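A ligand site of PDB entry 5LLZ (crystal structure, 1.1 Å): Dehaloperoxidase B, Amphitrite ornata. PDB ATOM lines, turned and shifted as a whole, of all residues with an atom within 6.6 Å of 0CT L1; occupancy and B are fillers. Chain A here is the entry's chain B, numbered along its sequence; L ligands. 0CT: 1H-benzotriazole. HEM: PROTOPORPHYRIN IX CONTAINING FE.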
ATOM      1  N   ALA A  17     -20.351  -9.664  -8.859  1.00  0.00           N
ATOM      2  CA  ALA A  17     -20.482 -10.985  -9.444  1.00  0.00           C
ATOM      3  C   ALA A  17     -21.174 -11.960  -8.502  1.00  0.00           C
ATOM      4  O   ALA A  17     -22.104 -12.656  -8.883  1.00  0.00           O
ATOM      5  CB  ALA A  17     -19.126 -11.492  -9.898  1.00  0.00           C
ATOM      6  N   ILE A  20     -25.009 -10.867  -7.861  1.00  0.00           N
ATOM      7  CA  ILE A  20     -25.885 -11.095  -9.005  1.00  0.00           C
ATOM      8  C   ILE A  20     -26.115 -12.619  -9.208  1.00  0.00           C
ATOM      9  O   ILE A  20     -27.230 -13.066  -9.461  1.00  0.00           O
ATOM     10  CB  ILE A  20     -25.397 -10.383 -10.298  1.00  0.00           C
ATOM     11  CG1 ILE A  20     -25.433  -8.868 -10.106  1.00  0.00           C
ATOM     12  CG2 ILE A  20     -26.222 -10.784 -11.512  1.00  0.00           C
ATOM     13  CD1 ILE A  20     -24.655  -8.023 -11.119  1.00  0.00           C
ATOM     14  N   PHE A  21     -25.025 -13.417  -9.090  1.00  0.00           N
ATOM     15  CA  PHE A  21     -25.188 -14.863  -9.241  1.00  0.00           C
ATOM     16  C   PHE A  21     -26.096 -15.435  -8.157  1.00  0.00           C
ATOM     17  O   PHE A  21     -26.971 -16.276  -8.457  1.00  0.00           O
ATOM     18  CB  PHE A  21     -23.825 -15.553  -9.217  1.00  0.00           C
ATOM     19  CG  PHE A  21     -23.837 -17.079  -9.504  1.00  0.00           C
ATOM     20  CD1 PHE A  21     -24.752 -17.698 -10.363  1.00  0.00           C
ATOM     21  CD2 PHE A  21     -22.960 -17.885  -8.832  1.00  0.00           C
ATOM     22  CE1 PHE A  21     -24.692 -19.074 -10.603  1.00  0.00           C
ATOM     23  CE2 PHE A  21     -22.874 -19.245  -9.106  1.00  0.00           C
ATOM     24  CZ  PHE A  21     -23.774 -19.824  -9.942  1.00  0.00           C
ATOM     25  N   PHE A  24     -29.709 -14.730  -9.070  1.00  0.00           N
ATOM     26  CA  PHE A  24     -30.145 -15.743 -10.051  1.00  0.00           C
ATOM     27  C   PHE A  24     -30.497 -17.092  -9.409  1.00  0.00           C
ATOM     28  O   PHE A  24     -31.581 -17.655  -9.671  1.00  0.00           O
ATOM     29  CB  PHE A  24     -29.019 -15.909 -11.144  1.00  0.00           C
ATOM     30  CG  PHE A  24     -29.185 -17.090 -12.040  1.00  0.00           C
ATOM     31  CD1 PHE A  24     -30.245 -17.156 -12.928  1.00  0.00           C
ATOM     32  CD2 PHE A  24     -28.242 -18.085 -12.061  1.00  0.00           C
ATOM     33  CE1 PHE A  24     -30.368 -18.225 -13.807  1.00  0.00           C
ATOM     34  CE2 PHE A  24     -28.364 -19.168 -12.949  1.00  0.00           C
ATOM     35  CZ  PHE A  24     -29.415 -19.237 -13.822  1.00  0.00           C
ATOM     36  N   PHE A  35     -25.080 -26.543 -11.036  1.00  0.00           N
ATOM     37  CA  PHE A  35     -24.103 -26.158 -10.052  1.00  0.00           C
ATOM     38  C   PHE A  35     -24.299 -27.079  -8.802  1.00  0.00           C
ATOM     39  O   PHE A  35     -24.534 -26.572  -7.656  1.00  0.00           O
ATOM     40  CB  PHE A  35     -24.234 -24.663  -9.691  1.00  0.00           C
ATOM     41  CG  PHE A  35     -24.102 -23.754 -10.836  1.00  0.00           C
ATOM     42  CD1 PHE A  35     -22.839 -23.422 -11.401  1.00  0.00           C
ATOM     43  CD2 PHE A  35     -25.240 -23.242 -11.455  1.00  0.00           C
ATOM     44  CE1 PHE A  35     -22.732 -22.567 -12.485  1.00  0.00           C
ATOM     45  CE2 PHE A  35     -25.135 -22.436 -12.579  1.00  0.00           C
ATOM     46  CZ  PHE A  35     -23.891 -22.092 -13.077  1.00  0.00           C
ATOM     47  N   TYR A  38     -22.917 -26.331  -5.143  1.00  0.00           N
ATOM     48  CA  TYR A  38     -23.481 -25.232  -4.323  1.00  0.00           C
ATOM     49  C   TYR A  38     -24.775 -25.578  -3.606  1.00  0.00           C
ATOM     50  O   TYR A  38     -25.338 -24.735  -2.913  1.00  0.00           O
ATOM     51  CB  TYR A  38     -23.665 -24.007  -5.239  1.00  0.00           C
ATOM     52  CG  TYR A  38     -22.393 -23.539  -5.912  1.00  0.00           C
ATOM     53  CD1 TYR A  38     -21.134 -23.761  -5.369  1.00  0.00           C
ATOM     54  CD2 TYR A  38     -22.455 -22.801  -7.109  1.00  0.00           C
ATOM     55  CE1 TYR A  38     -19.986 -23.291  -5.974  1.00  0.00           C
ATOM     56  CE2 TYR A  38     -21.302 -22.355  -7.720  1.00  0.00           C
ATOM     57  CZ  TYR A  38     -20.083 -22.604  -7.191  1.00  0.00           C
ATOM     58  OH  TYR A  38     -18.984 -22.093  -7.842  1.00  0.00           O
ATOM     59  N   HIS A  55     -14.526 -18.278  -8.978  1.00  0.00           N
ATOM     60  CA  HIS A  55     -15.275 -18.683 -10.149  1.00  0.00           C
ATOM     61  C   HIS A  55     -16.174 -17.530 -10.702  1.00  0.00           C
ATOM     62  O   HIS A  55     -16.168 -17.253 -11.933  1.00  0.00           O
ATOM     63  CB  HIS A  55     -16.134 -19.899  -9.774  1.00  0.00           C
ATOM     64  CG  HIS A  55     -17.180 -20.217 -10.762  1.00  0.00           C
ATOM     65  ND1 HIS A  55     -16.893 -20.708 -12.018  1.00  0.00           N
ATOM     66  CD2 HIS A  55     -18.532 -20.067 -10.716  1.00  0.00           C
ATOM     67  CE1 HIS A  55     -18.017 -20.883 -12.693  1.00  0.00           C
ATOM     68  NE2 HIS A  55     -19.020 -20.507 -11.928  1.00  0.00           N
ATOM     69  N   THR A  56     -16.985 -16.917  -9.827  1.00  0.00           N
ATOM     70  CA  THR A  56     -17.928 -15.862 -10.279  1.00  0.00           C
ATOM     71  C   THR A  56     -17.214 -14.661 -10.854  1.00  0.00           C
ATOM     72  O   THR A  56     -17.659 -14.077 -11.879  1.00  0.00           O
ATOM     73  CB  THR A  56     -18.951 -15.409  -9.172  1.00  0.00           C
ATOM     74  OG1 THR A  56     -18.299 -14.871  -8.011  1.00  0.00           O
ATOM     75  CG2 THR A  56     -19.907 -16.558  -8.789  1.00  0.00           C
ATOM     76  N   VAL A  59     -16.258 -15.481 -14.419  1.00  0.00           N
ATOM     77  CA  VAL A  59     -17.456 -15.419 -15.225  1.00  0.00           C
ATOM     78  C   VAL A  59     -17.804 -13.986 -15.632  1.00  0.00           C
ATOM     79  O   VAL A  59     -18.057 -13.661 -16.824  1.00  0.00           O
ATOM     80  CB  VAL A  59     -18.662 -16.085 -14.473  1.00  0.00           C
ATOM     81  CG1 VAL A  59     -19.982 -15.782 -15.136  1.00  0.00           C
ATOM     82  CG2 VAL A  59     -18.441 -17.588 -14.285  1.00  0.00           C
ATOM     83  N   PHE A  60     -17.870 -13.119 -14.616  1.00  0.00           N
ATOM     84  CA  PHE A  60     -18.263 -11.734 -14.874  1.00  0.00           C
ATOM     85  C   PHE A  60     -17.195 -10.925 -15.611  1.00  0.00           C
ATOM     86  O   PHE A  60     -17.542  -9.987 -16.370  1.00  0.00           O
ATOM     87  CB  PHE A  60     -18.781 -11.041 -13.593  1.00  0.00           C
ATOM     88  CG  PHE A  60     -20.221 -11.387 -13.317  1.00  0.00           C
ATOM     89  CD1 PHE A  60     -20.612 -12.660 -12.851  1.00  0.00           C
ATOM     90  CD2 PHE A  60     -21.240 -10.430 -13.508  1.00  0.00           C
ATOM     91  CE1 PHE A  60     -21.955 -12.965 -12.648  1.00  0.00           C
ATOM     92  CE2 PHE A  60     -22.570 -10.731 -13.278  1.00  0.00           C
ATOM     93  CZ  PHE A  60     -22.934 -11.989 -12.846  1.00  0.00           C
ATOM     94  N   MET A  63     -18.160 -11.776 -19.088  1.00  0.00           N
ATOM     95  CA  MET A  63     -19.412 -11.075 -19.415  1.00  0.00           C
ATOM     96  C   MET A  63     -19.131  -9.586 -19.763  1.00  0.00           C
ATOM     97  O   MET A  63     -19.734  -9.022 -20.688  1.00  0.00           O
ATOM     98  CB  MET A  63     -20.445 -11.151 -18.237  1.00  0.00           C
ATOM     99  CG  MET A  63     -21.828 -10.666 -18.673  1.00  0.00           C
ATOM    100  SD  MET A  63     -22.979 -10.458 -17.267  1.00  0.00           S
ATOM    101  CE  MET A  63     -23.193 -12.139 -16.709  1.00  0.00           C
ATOM    102  N   HIS A  89     -20.074 -25.144 -21.007  1.00  0.00           N
ATOM    103  CA  HIS A  89     -21.435 -24.825 -21.406  1.00  0.00           C
ATOM    104  C   HIS A  89     -22.134 -25.905 -22.260  1.00  0.00           C
ATOM    105  O   HIS A  89     -23.242 -25.662 -22.808  1.00  0.00           O
ATOM    106  CB  HIS A  89     -21.430 -23.457 -22.095  1.00  0.00           C
ATOM    107  CG  HIS A  89     -21.127 -22.294 -21.195  1.00  0.00           C
ATOM    108  ND1 HIS A  89     -20.848 -21.030 -21.684  1.00  0.00           N
ATOM    109  CD2 HIS A  89     -21.083 -22.190 -19.829  1.00  0.00           C
ATOM    110  CE1 HIS A  89     -20.681 -20.205 -20.644  1.00  0.00           C
ATOM    111  NE2 HIS A  89     -20.810 -20.882 -19.521  1.00  0.00           N
ATOM    112  N   LEU A  92     -26.155 -26.652 -22.099  1.00  0.00           N
ATOM    113  CA  LEU A  92     -27.020 -25.494 -21.823  1.00  0.00           C
ATOM    114  C   LEU A  92     -27.929 -25.204 -22.999  1.00  0.00           C
ATOM    115  O   LEU A  92     -27.634 -25.588 -24.121  1.00  0.00           O
ATOM    116  CB  LEU A  92     -26.226 -24.218 -21.437  1.00  0.00           C
ATOM    117  CG  LEU A  92     -25.302 -24.381 -20.224  1.00  0.00           C
ATOM    118  CD1 LEU A  92     -24.547 -23.081 -19.955  1.00  0.00           C
ATOM    119  CD2 LEU A  92     -26.013 -24.848 -18.971  1.00  0.00           C
ATOM    120  N   PHE A  97     -29.696 -18.731 -20.140  1.00  0.00           N
ATOM    121  CA  PHE A  97     -29.204 -17.381 -20.289  1.00  0.00           C
ATOM    122  C   PHE A  97     -30.302 -16.377 -20.127  1.00  0.00           C
ATOM    123  O   PHE A  97     -30.099 -15.306 -19.520  1.00  0.00           O
ATOM    124  CB  PHE A  97     -28.434 -17.218 -21.628  1.00  0.00           C
ATOM    125  CG  PHE A  97     -27.142 -17.979 -21.735  1.00  0.00           C
ATOM    126  CD1 PHE A  97     -27.098 -19.373 -21.968  1.00  0.00           C
ATOM    127  CD2 PHE A  97     -25.950 -17.318 -21.612  1.00  0.00           C
ATOM    128  CE1 PHE A  97     -25.887 -20.034 -22.032  1.00  0.00           C
ATOM    129  CE2 PHE A  97     -24.737 -17.994 -21.652  1.00  0.00           C
ATOM    130  CZ  PHE A  97     -24.708 -19.326 -21.887  1.00  0.00           C
ATOM    131  N   LEU A 100     -30.829 -15.924 -16.412  1.00  0.00           N
ATOM    132  CA  LEU A 100     -29.734 -15.167 -15.796  1.00  0.00           C
ATOM    133  C   LEU A 100     -29.941 -13.638 -16.002  1.00  0.00           C
ATOM    134  O   LEU A 100     -29.766 -12.867 -15.029  1.00  0.00           O
ATOM    135  CB  LEU A 100     -28.395 -15.596 -16.384  1.00  0.00           C
ATOM    136  CG  LEU A 100     -27.148 -14.774 -16.005  1.00  0.00           C
ATOM    137  CD1 LEU A 100     -26.891 -14.781 -14.464  1.00  0.00           C
ATOM    138  CD2 LEU A 100     -25.883 -15.222 -16.741  1.00  0.00           C
HETATM  139  NAF 0CT L   1     -21.236 -19.413 -15.628  1.00  0.00           N
HETATM  140  CAH 0CT L   1     -22.038 -18.518 -14.995  1.00  0.00           C
HETATM  141  CAC 0CT L   1     -22.876 -17.417 -15.517  1.00  0.00           C
HETATM  142  CAA 0CT L   1     -23.603 -16.541 -14.558  1.00  0.00           C
HETATM  143  CAB 0CT L   1     -23.430 -16.716 -13.100  1.00  0.00           C
HETATM  144  CAD 0CT L   1     -22.569 -17.794 -12.581  1.00  0.00           C
HETATM  145  CAI 0CT L   1     -21.899 -18.663 -13.532  1.00  0.00           C
HETATM  146  NAG 0CT L   1     -21.076 -19.666 -13.373  1.00  0.00           N
HETATM  147  NAE 0CT L   1     -20.662 -20.138 -14.600  1.00  0.00           N
HETATM  148  CHA HEM L   2     -18.195 -21.898 -16.360  1.00  0.00           C
HETATM  149  CHB HEM L   2     -18.734 -17.519 -18.434  1.00  0.00           C
HETATM  150  CHC HEM L   2     -23.554 -18.098 -18.522  1.00  0.00           C
HETATM  151  CHD HEM L   2     -23.057 -22.496 -16.507  1.00  0.00           C
HETATM  152  C1A HEM L   2     -17.934 -20.607 -16.881  1.00  0.00           C
HETATM  153  C2A HEM L   2     -16.613 -19.992 -16.897  1.00  0.00           C
HETATM  154  C3A HEM L   2     -16.744 -18.794 -17.516  1.00  0.00           C
HETATM  155  C4A HEM L   2     -18.163 -18.642 -17.857  1.00  0.00           C
HETATM  156  CMA HEM L   2     -15.625 -17.779 -17.785  1.00  0.00           C
HETATM  157  CAA HEM L   2     -15.295 -20.556 -16.338  1.00  0.00           C
HETATM  158  CBA HEM L   2     -14.992 -19.911 -14.952  1.00  0.00           C
HETATM  159  CGA HEM L   2     -13.892 -20.473 -14.093  1.00  0.00           C
HETATM  160  O1A HEM L   2     -14.108 -20.909 -12.889  1.00  0.00           O
HETATM  161  O2A HEM L   2     -12.752 -20.483 -14.588  1.00  0.00           O
HETATM  162  C1B HEM L   2     -20.127 -17.301 -18.619  1.00  0.00           C
HETATM  163  C2B HEM L   2     -20.662 -16.069 -19.181  1.00  0.00           C
HETATM  164  C3B HEM L   2     -22.031 -16.207 -19.223  1.00  0.00           C
HETATM  165  C4B HEM L   2     -22.274 -17.575 -18.676  1.00  0.00           C
HETATM  166  CMB HEM L   2     -19.860 -14.839 -19.527  1.00  0.00           C
HETATM  167  CAB HEM L   2     -23.111 -15.294 -19.696  1.00  0.00           C
HETATM  168  CBB HEM L   2     -22.931 -14.274 -20.582  1.00  0.00           C
HETATM  169  C1C HEM L   2     -23.844 -19.353 -17.951  1.00  0.00           C
HETATM  170  C2C HEM L   2     -25.152 -19.790 -17.666  1.00  0.00           C
HETATM  171  C3C HEM L   2     -25.047 -21.047 -17.040  1.00  0.00           C
HETATM  172  C4C HEM L   2     -23.623 -21.345 -17.008  1.00  0.00           C
HETATM  173  CMC HEM L   2     -26.491 -19.046 -17.968  1.00  0.00           C
HETATM  174  CAC HEM L   2     -26.097 -21.904 -16.443  1.00  0.00           C
HETATM  175  CBC HEM L   2     -27.272 -21.456 -15.930  1.00  0.00           C
HETATM  176  C1D HEM L   2     -21.670 -22.713 -16.346  1.00  0.00           C
HETATM  177  C2D HEM L   2     -21.125 -23.954 -15.757  1.00  0.00           C
HETATM  178  C3D HEM L   2     -19.784 -23.795 -15.675  1.00  0.00           C
HETATM  179  C4D HEM L   2     -19.484 -22.463 -16.282  1.00  0.00           C
HETATM  180  CMD HEM L   2     -21.894 -25.142 -15.228  1.00  0.00           C
HETATM  181  CAD HEM L   2     -18.799 -24.787 -15.103  1.00  0.00           C
HETATM  182  CBD HEM L   2     -18.643 -24.529 -13.597  1.00  0.00           C
HETATM  183  CGD HEM L   2     -17.133 -24.528 -13.451  1.00  0.00           C
HETATM  184  O1D HEM L   2     -16.364 -23.515 -13.789  1.00  0.00           O
HETATM  185  O2D HEM L   2     -16.716 -25.643 -13.058  1.00  0.00           O
HETATM  186  NA  HEM L   2     -18.879 -19.770 -17.453  1.00  0.00           N
HETATM  187  NB  HEM L   2     -21.110 -18.181 -18.351  1.00  0.00           N
HETATM  188  NC  HEM L   2     -22.900 -20.284 -17.522  1.00  0.00           N
HETATM  189  ND  HEM L   2     -20.648 -21.857 -16.716  1.00  0.00           N
HETATM  190 FE   HEM L   2     -20.883 -20.058 -17.536  1.00  0.00          FE
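A nitrogen (NAG) of 0CT L1 is in hydrogen-bond range of a ring nitrogen (NE2) of His 55 (2.6 Å).
O1A of HEM L2 is in hydrogen-bond range of ND1 of His 55 (2.9 Å).
NE2 of His 89 binds FE of HEM L2, 2.2 Å away.
NAF of 0CT L1 binds FE of HEM L2 (2.0 Å).
CD1 of Phe 21 touches CAD of 0CT L1, at 3.1 Å.
Phe 35 touches 0CT L1.
CG1 of Val 59 touches CAC of 0CT L1, at 3.3 Å.
Leu 100 touches 0CT L1.
Hydrophobic or aromatic side chains that line 0CT L1: Phe 21, Phe 35, His 55, Val 59 and Leu 100.
Five residues have an atom within 4 Å of 0CT L1: Phe 21, Phe 35, His 55, Val 59 and Leu 100.
The nearest printed residue that does not touch 0CT L1 is Phe 60 (4.1 Å).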
